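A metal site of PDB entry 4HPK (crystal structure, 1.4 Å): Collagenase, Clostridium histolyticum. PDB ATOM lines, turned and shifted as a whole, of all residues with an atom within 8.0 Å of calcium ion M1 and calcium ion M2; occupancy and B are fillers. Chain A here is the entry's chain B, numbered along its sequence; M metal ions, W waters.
The side-chain amide nitrogen (ND2) of Asn 13 lies close to the side-chain carboxylate (OE2) of Glu 9 (2.9 Å). The backbone NH of Asp 14 lies within hydrogen-bond range of the side-chain amide oxygen of Asn 12. The backbone NH of Glu 9 is in hydrogen-bond range of the backbone carbonyl oxygen of Gln 30 (3.0 Å). The backbone NH (N) of Tyr 41 is in hydrogen-bond range of the backbone carbonyl oxygen (O) of Asn 13. The backbone NH (N) of Asp 40 is in hydrogen-bond range of the backbone carbonyl oxygen (O) of Val 103, 2.8 Å away. The side-chain hydroxyl (OG1) of Thr 20 lies within hydrogen-bond range of the side-chain amide nitrogen (ND2) of Asn 13 (3.5 Å). The side-chain carboxylate (OD2) of Asp 40 lies close to the side-chain hydroxyl (OH) of Tyr 112 (2.6 Å).
Within 4 Å of calcium ion M2: Glu 11, Asn 13, Asp 14, Asp 37, Arg 39 and Asp 40. Along chain A the residues within 4 Å of calcium ion M2 span positions 11 to 40.
Calcium ion M1 is bound by OD2 of Asp 37 (2.3 Å), OE2 of Glu 11 (2.3 Å), O of Ser 32 (2.3 Å), water W1 (2.4 Å), OE1 of Glu 9 (2.4 Å), OD1 of Asp 40 (2.5 Å), OE2 of Glu 9 (2.5 Å) and OD2 of Asp 40 (2.6 Å).
Calcium ion M2 is bound by the backbone carbonyl oxygen (O) of Arg 39 (2.3 Å), the side-chain carboxylate (OD2) of Asp 14 (2.3 Å), the side-chain amide oxygen (OD1) of Asn 13 (2.3 Å), the side-chain carboxylate (OD1) of Asp 40 (2.4 Å), the side-chain carboxylate (OE2) of Glu 11 (2.4 Å), the side-chain carboxylate (OD1) of Asp 37 (2.4 Å) and the side-chain carboxylate (OE1) of Glu 11 (2.6 Å). Calcium ion M2 has seven donor atoms within binding distance.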
ATOM      1  N   GLU A   9      20.863   6.580   8.168  1.00  0.00           N
ATOM      2  CA  GLU A   9      21.507   6.336   9.456  1.00  0.00           C
ATOM      3  C   GLU A   9      21.672   4.833   9.684  1.00  0.00           C
ATOM      4  O   GLU A   9      20.952   4.021   9.096  1.00  0.00           O
ATOM      5  CB  GLU A   9      20.661   6.920  10.583  1.00  0.00           C
ATOM      6  CG  GLU A   9      19.250   6.336  10.656  1.00  0.00           C
ATOM      7  CD  GLU A   9      18.534   6.613  11.952  1.00  0.00           C
ATOM      8  OE1 GLU A   9      17.281   6.720  11.934  1.00  0.00           O
ATOM      9  OE2 GLU A   9      19.203   6.684  13.008  1.00  0.00           O
ATOM     10  N   LYS A  10      22.602   4.484  10.581  1.00  0.00           N
ATOM     11  CA  LYS A  10      22.838   3.076  10.942  1.00  0.00           C
ATOM     12  C   LYS A  10      22.650   2.832  12.452  1.00  0.00           C
ATOM     13  O   LYS A  10      23.546   3.105  13.241  1.00  0.00           O
ATOM     14  CB  LYS A  10      24.246   2.647  10.524  1.00  0.00           C
ATOM     15  CG  LYS A  10      24.532   2.814   9.039  1.00  0.00           C
ATOM     16  CD  LYS A  10      25.884   2.249   8.662  1.00  0.00           C
ATOM     17  CE  LYS A  10      26.141   2.326   7.169  1.00  0.00           C
ATOM     18  NZ  LYS A  10      26.390   3.711   6.719  1.00  0.00           N
ATOM     19  N   GLU A  11      21.476   2.329  12.832  1.00  0.00           N
ATOM     20  CA  GLU A  11      21.228   1.947  14.235  1.00  0.00           C
ATOM     21  C   GLU A  11      22.018   0.674  14.553  1.00  0.00           C
ATOM     22  O   GLU A  11      22.270  -0.116  13.640  1.00  0.00           O
ATOM     23  CB  GLU A  11      19.749   1.661  14.467  1.00  0.00           C
ATOM     24  CG  GLU A  11      18.842   2.881  14.339  1.00  0.00           C
ATOM     25  CD  GLU A  11      18.966   3.874  15.493  1.00  0.00           C
ATOM     26  OE1 GLU A  11      19.654   3.594  16.515  1.00  0.00           O
ATOM     27  OE2 GLU A  11      18.368   4.966  15.351  1.00  0.00           O
ATOM     28  N   ASN A  12      22.417   0.451  15.812  1.00  0.00           N
ATOM     29  CA  ASN A  12      22.239   1.341  16.953  1.00  0.00           C
ATOM     30  C   ASN A  12      23.249   2.485  16.865  1.00  0.00           C
ATOM     31  O   ASN A  12      24.433   2.258  16.677  1.00  0.00           O
ATOM     32  CB  ASN A  12      22.474   0.531  18.249  1.00  0.00           C
ATOM     33  CG  ASN A  12      22.242   1.328  19.544  1.00  0.00           C
ATOM     34  OD1 ASN A  12      22.394   2.534  19.599  1.00  0.00           O
ATOM     35  ND2 ASN A  12      21.912   0.600  20.609  1.00  0.00           N
ATOM     36  N   ASN A  13      22.768   3.721  16.970  1.00  0.00           N
ATOM     37  CA  ASN A  13      23.650   4.899  16.980  1.00  0.00           C
ATOM     38  C   ASN A  13      23.365   5.818  18.169  1.00  0.00           C
ATOM     39  O   ASN A  13      23.507   7.022  18.068  1.00  0.00           O
ATOM     40  CB  ASN A  13      23.522   5.667  15.662  1.00  0.00           C
ATOM     41  CG  ASN A  13      22.099   6.077  15.374  1.00  0.00           C
ATOM     42  OD1 ASN A  13      21.245   6.063  16.265  1.00  0.00           O
ATOM     43  ND2 ASN A  13      21.824   6.418  14.118  1.00  0.00           N
ATOM     44  N   ASP A  14      22.982   5.243  19.312  1.00  0.00           N
ATOM     45  CA  ASP A  14      22.488   6.054  20.428  1.00  0.00           C
ATOM     46  C   ASP A  14      23.582   6.680  21.307  1.00  0.00           C
ATOM     47  O   ASP A  14      23.278   7.511  22.163  1.00  0.00           O
ATOM     48  CB  ASP A  14      21.528   5.236  21.296  1.00  0.00           C
ATOM     49  CG  ASP A  14      20.304   4.754  20.524  1.00  0.00           C
ATOM     50  OD1 ASP A  14      19.523   3.971  21.115  1.00  0.00           O
ATOM     51  OD2 ASP A  14      20.093   5.142  19.349  1.00  0.00           O
ATOM     52  N   SER A  15      24.838   6.295  21.093  1.00  0.00           N
ATOM     53  CA  SER A  15      25.969   6.882  21.837  1.00  0.00           C
ATOM     54  C   SER A  15      27.068   7.324  20.889  1.00  0.00           C
ATOM     55  O   SER A  15      27.085   6.933  19.721  1.00  0.00           O
ATOM     56  CB  SER A  15      26.534   5.859  22.816  1.00  0.00           C
ATOM     57  OG  SER A  15      27.009   4.712  22.131  1.00  0.00           O
ATOM     58  N   LYS A  18      29.003   4.797  18.923  1.00  0.00           N
ATOM     59  CA  LYS A  18      28.243   4.106  17.888  1.00  0.00           C
ATOM     60  C   LYS A  18      27.740   5.057  16.788  1.00  0.00           C
ATOM     61  O   LYS A  18      26.873   4.705  15.993  1.00  0.00           O
ATOM     62  CB  LYS A  18      27.046   3.385  18.520  1.00  0.00           C
ATOM     63  CG  LYS A  18      27.406   2.369  19.610  1.00  0.00           C
ATOM     64  CD  LYS A  18      26.143   1.827  20.279  1.00  0.00           C
ATOM     65  CE  LYS A  18      26.467   0.943  21.484  1.00  0.00           C
ATOM     66  NZ  LYS A  18      25.223   0.472  22.168  1.00  0.00           N
ATOM     67  N   THR A  20      26.893   7.239  13.538  1.00  0.00           N
ATOM     68  CA  THR A  20      26.911   7.011  12.094  1.00  0.00           C
ATOM     69  C   THR A  20      27.798   8.053  11.438  1.00  0.00           C
ATOM     70  O   THR A  20      27.613   9.249  11.632  1.00  0.00           O
ATOM     71  CB  THR A  20      25.506   7.107  11.487  1.00  0.00           C
ATOM     72  OG1 THR A  20      24.637   6.169  12.135  1.00  0.00           O
ATOM     73  CG2 THR A  20      25.533   6.854   9.978  1.00  0.00           C
ATOM     74  N   GLN A  30      19.504  10.558   6.245  1.00  0.00           N
ATOM     75  CA  GLN A  30      18.086  10.343   6.452  1.00  0.00           C
ATOM     76  C   GLN A  30      17.914   9.531   7.707  1.00  0.00           C
ATOM     77  O   GLN A  30      18.514   8.475   7.849  1.00  0.00           O
ATOM     78  CB  GLN A  30      17.487   9.612   5.261  1.00  0.00           C
ATOM     79  CG  GLN A  30      17.619  10.438   3.991  1.00  0.00           C
ATOM     80  CD  GLN A  30      17.151   9.714   2.745  1.00  0.00           C
ATOM     81  OE1 GLN A  30      17.504   8.565   2.520  1.00  0.00           O
ATOM     82  NE2 GLN A  30      16.363  10.407   1.935  1.00  0.00           N
ATOM     83  N   GLY A  31      17.117  10.036   8.642  1.00  0.00           N
ATOM     84  CA  GLY A  31      16.922   9.354   9.901  1.00  0.00           C
ATOM     85  C   GLY A  31      15.506   9.462  10.424  1.00  0.00           C
ATOM     86  O   GLY A  31      14.671  10.216   9.899  1.00  0.00           O
ATOM     87  N   SER A  32      15.247   8.671  11.458  1.00  0.00           N
ATOM     88  CA  SER A  32      13.959   8.704  12.129  1.00  0.00           C
ATOM     89  C   SER A  32      14.176   8.564  13.609  1.00  0.00           C
ATOM     90  O   SER A  32      15.118   7.895  14.069  1.00  0.00           O
ATOM     91  CB  SER A  32      13.035   7.578  11.640  1.00  0.00           C
ATOM     92  OG  SER A  32      13.443   6.317  12.085  1.00  0.00           O
ATOM     93  N   LEU A  33      13.280   9.201  14.375  1.00  0.00           N
ATOM     94  CA  LEU A  33      13.258   9.109  15.823  1.00  0.00           C
ATOM     95  C   LEU A  33      11.839   8.738  16.240  1.00  0.00           C
ATOM     96  O   LEU A  33      11.088   9.571  16.731  1.00  0.00           O
ATOM     97  CB  LEU A  33      13.669  10.438  16.443  1.00  0.00           C
ATOM     98  CG  LEU A  33      15.151  10.777  16.227  1.00  0.00           C
ATOM     99  CD1 LEU A  33      15.375  12.227  16.551  1.00  0.00           C
ATOM    100  CD2 LEU A  33      16.070   9.890  17.062  1.00  0.00           C
ATOM    101  N   LEU A  34      11.463   7.485  15.993  1.00  0.00           N
ATOM    102  CA  LEU A  34      10.123   6.981  16.309  1.00  0.00           C
ATOM    103  C   LEU A  34      10.077   6.254  17.644  1.00  0.00           C
ATOM    104  O   LEU A  34      10.921   5.425  17.934  1.00  0.00           O
ATOM    105  CB  LEU A  34       9.676   6.015  15.201  1.00  0.00           C
ATOM    106  CG  LEU A  34       9.744   6.514  13.772  1.00  0.00           C
ATOM    107  CD1 LEU A  34       9.251   5.410  12.821  1.00  0.00           C
ATOM    108  CD2 LEU A  34       8.944   7.787  13.547  1.00  0.00           C
ATOM    109  N   ASP A  36      10.585   4.925  21.163  1.00  0.00           N
ATOM    110  CA  ASP A  36      11.692   4.966  22.105  1.00  0.00           C
ATOM    111  C   ASP A  36      13.044   5.314  21.502  1.00  0.00           C
ATOM    112  O   ASP A  36      13.993   5.533  22.250  1.00  0.00           O
ATOM    113  CB  ASP A  36      11.787   3.649  22.884  1.00  0.00           C
ATOM    114  CG  ASP A  36      10.608   3.428  23.817  1.00  0.00           C
ATOM    115  OD1 ASP A  36       9.953   4.405  24.231  1.00  0.00           O
ATOM    116  OD2 ASP A  36      10.355   2.254  24.137  1.00  0.00           O
ATOM    117  N   ASP A  37      13.156   5.363  20.171  1.00  0.00           N
ATOM    118  CA  ASP A  37      14.385   5.838  19.544  1.00  0.00           C
ATOM    119  C   ASP A  37      14.391   7.361  19.598  1.00  0.00           C
ATOM    120  O   ASP A  37      13.696   8.010  18.835  1.00  0.00           O
ATOM    121  CB  ASP A  37      14.488   5.342  18.093  1.00  0.00           C
ATOM    122  CG  ASP A  37      15.797   5.749  17.425  1.00  0.00           C
ATOM    123  OD1 ASP A  37      16.862   5.706  18.083  1.00  0.00           O
ATOM    124  OD2 ASP A  37      15.760   6.103  16.221  1.00  0.00           O
ATOM    125  N   SER A  38      15.152   7.908  20.539  1.00  0.00           N
ATOM    126  CA  SER A  38      15.110   9.354  20.769  1.00  0.00           C
ATOM    127  C   SER A  38      16.438  10.060  20.537  1.00  0.00           C
ATOM    128  O   SER A  38      16.505  11.272  20.659  1.00  0.00           O
ATOM    129  CB  SER A  38      14.626   9.659  22.178  1.00  0.00           C
ATOM    130  OG  SER A  38      15.560   9.160  23.101  1.00  0.00           O
ATOM    131  N   ARG A  39      17.471   9.293  20.197  1.00  0.00           N
ATOM    132  CA  ARG A  39      18.787   9.851  19.921  1.00  0.00           C
ATOM    133  C   ARG A  39      19.428   9.139  18.743  1.00  0.00           C
ATOM    134  O   ARG A  39      19.441   7.890  18.695  1.00  0.00           O
ATOM    135  CB  ARG A  39      19.715   9.670  21.112  1.00  0.00           C
ATOM    136  CG  ARG A  39      19.237  10.254  22.428  1.00  0.00           C
ATOM    137  CD  ARG A  39      19.900   9.560  23.591  1.00  0.00           C
ATOM    138  NE  ARG A  39      21.369   9.561  23.510  1.00  0.00           N
ATOM    139  CZ  ARG A  39      22.169  10.475  24.071  1.00  0.00           C
ATOM    140  NH1 ARG A  39      21.663  11.496  24.747  1.00  0.00           N
ATOM    141  NH2 ARG A  39      23.496  10.356  23.950  1.00  0.00           N
ATOM    142  N   ASP A  40      19.957   9.919  17.812  1.00  0.00           N
ATOM    143  CA  ASP A  40      20.751   9.426  16.672  1.00  0.00           C
ATOM    144  C   ASP A  40      22.046  10.224  16.645  1.00  0.00           C
ATOM    145  O   ASP A  40      22.036  11.435  16.397  1.00  0.00           O
ATOM    146  CB  ASP A  40      20.006   9.651  15.341  1.00  0.00           C
ATOM    147  CG  ASP A  40      18.768   8.758  15.169  1.00  0.00           C
ATOM    148  OD1 ASP A  40      18.619   7.751  15.901  1.00  0.00           O
ATOM    149  OD2 ASP A  40      17.942   9.062  14.279  1.00  0.00           O
ATOM    150  N   TYR A  41      23.159   9.542  16.899  1.00  0.00           N
ATOM    151  CA  TYR A  41      24.465  10.171  16.942  1.00  0.00           C
ATOM    152  C   TYR A  41      25.134  10.019  15.564  1.00  0.00           C
ATOM    153  O   TYR A  41      25.085   8.946  14.954  1.00  0.00           O
ATOM    154  CB  TYR A  41      25.352   9.566  18.052  1.00  0.00           C
ATOM    155  CG  TYR A  41      25.980  10.594  18.980  1.00  0.00           C
ATOM    156  CD1 TYR A  41      25.867  10.485  20.361  1.00  0.00           C
ATOM    157  CD2 TYR A  41      26.629  11.691  18.457  1.00  0.00           C
ATOM    158  CE1 TYR A  41      26.434  11.435  21.202  1.00  0.00           C
ATOM    159  CE2 TYR A  41      27.179  12.651  19.287  1.00  0.00           C
ATOM    160  CZ  TYR A  41      27.090  12.521  20.658  1.00  0.00           C
ATOM    161  OH  TYR A  41      27.648  13.489  21.453  1.00  0.00           O
ATOM    162  N   TYR A  42      25.721  11.122  15.101  1.00  0.00           N
ATOM    163  CA  TYR A  42      26.513  11.167  13.885  1.00  0.00           C
ATOM    164  C   TYR A  42      27.922  11.684  14.208  1.00  0.00           C
ATOM    165  O   TYR A  42      28.150  12.309  15.233  1.00  0.00           O
ATOM    166  CB  TYR A  42      25.859  12.095  12.858  1.00  0.00           C
ATOM    167  CG  TYR A  42      24.510  11.623  12.413  1.00  0.00           C
ATOM    168  CD1 TYR A  42      23.355  12.013  13.084  1.00  0.00           C
ATOM    169  CD2 TYR A  42      24.374  10.778  11.310  1.00  0.00           C
ATOM    170  CE1 TYR A  42      22.113  11.572  12.665  1.00  0.00           C
ATOM    171  CE2 TYR A  42      23.138  10.342  10.885  1.00  0.00           C
ATOM    172  CZ  TYR A  42      22.007  10.728  11.562  1.00  0.00           C
ATOM    173  OH  TYR A  42      20.774  10.288  11.120  1.00  0.00           O
ATOM    174  N   LEU A 102      24.902  15.049  17.811  1.00  0.00           N
ATOM    175  CA  LEU A 102      23.820  14.289  18.398  1.00  0.00           C
ATOM    176  C   LEU A 102      22.507  14.929  17.986  1.00  0.00           C
ATOM    177  O   LEU A 102      22.257  16.092  18.321  1.00  0.00           O
ATOM    178  CB  LEU A 102      23.932  14.303  19.936  1.00  0.00           C
ATOM    179  CG  LEU A 102      22.750  13.690  20.701  1.00  0.00           C
ATOM    180  CD1 LEU A 102      22.575  12.212  20.355  1.00  0.00           C
ATOM    181  CD2 LEU A 102      22.937  13.911  22.212  1.00  0.00           C
ATOM    182  N   VAL A 103      21.692  14.179  17.259  1.00  0.00           N
ATOM    183  CA  VAL A 103      20.307  14.567  16.975  1.00  0.00           C
ATOM    184  C   VAL A 103      19.426  13.878  18.014  1.00  0.00           C
ATOM    185  O   VAL A 103      19.490  12.666  18.182  1.00  0.00           O
ATOM    186  CB  VAL A 103      19.892  14.151  15.539  1.00  0.00           C
ATOM    187  CG1 VAL A 103      18.440  14.532  15.263  1.00  0.00           C
ATOM    188  CG2 VAL A 103      20.807  14.810  14.494  1.00  0.00           C
ATOM    189  N   GLY A 110       9.138  11.438  14.735  1.00  0.00           N
ATOM    190  CA  GLY A 110       9.159  11.776  13.335  1.00  0.00           C
ATOM    191  C   GLY A 110      10.475  11.488  12.658  1.00  0.00           C
ATOM    192  O   GLY A 110      11.423  10.989  13.262  1.00  0.00           O
ATOM    193  N   ASN A 111      10.492  11.842  11.374  1.00  0.00           N
ATOM    194  CA  ASN A 111      11.637  11.661  10.494  1.00  0.00           C
ATOM    195  C   ASN A 111      12.275  13.001  10.197  1.00  0.00           C
ATOM    196  O   ASN A 111      11.665  14.067  10.354  1.00  0.00           O
ATOM    197  CB  ASN A 111      11.192  11.026   9.178  1.00  0.00           C
ATOM    198  CG  ASN A 111      10.580   9.653   9.367  1.00  0.00           C
ATOM    199  OD1 ASN A 111      10.854   8.971  10.346  1.00  0.00           O
ATOM    200  ND2 ASN A 111       9.739   9.253   8.417  1.00  0.00           N
ATOM    201  N   TYR A 112      13.535  12.961   9.772  1.00  0.00           N
ATOM    202  CA  TYR A 112      14.293  14.160   9.500  1.00  0.00           C
ATOM    203  C   TYR A 112      15.379  13.855   8.459  1.00  0.00           C
ATOM    204  O   TYR A 112      15.688  12.696   8.192  1.00  0.00           O
ATOM    205  CB  TYR A 112      14.935  14.706  10.801  1.00  0.00           C
ATOM    206  CG  TYR A 112      15.952  13.757  11.372  1.00  0.00           C
ATOM    207  CD1 TYR A 112      17.281  13.798  10.958  1.00  0.00           C
ATOM    208  CD2 TYR A 112      15.573  12.760  12.241  1.00  0.00           C
ATOM    209  CE1 TYR A 112      18.205  12.888  11.442  1.00  0.00           C
ATOM    210  CE2 TYR A 112      16.486  11.838  12.719  1.00  0.00           C
ATOM    211  CZ  TYR A 112      17.805  11.904  12.316  1.00  0.00           C
ATOM    212  OH  TYR A 112      18.732  10.992  12.783  1.00  0.00           O
HETATM  213 CA    CA M   1      17.060   6.626  14.357  1.00  0.00          CA
HETATM  214 CA    CA M   2      19.183   5.986  17.370  1.00  0.00          CA
HETATM  215  O   HOH W   1      15.834   4.672  13.600  1.00  0.00           O
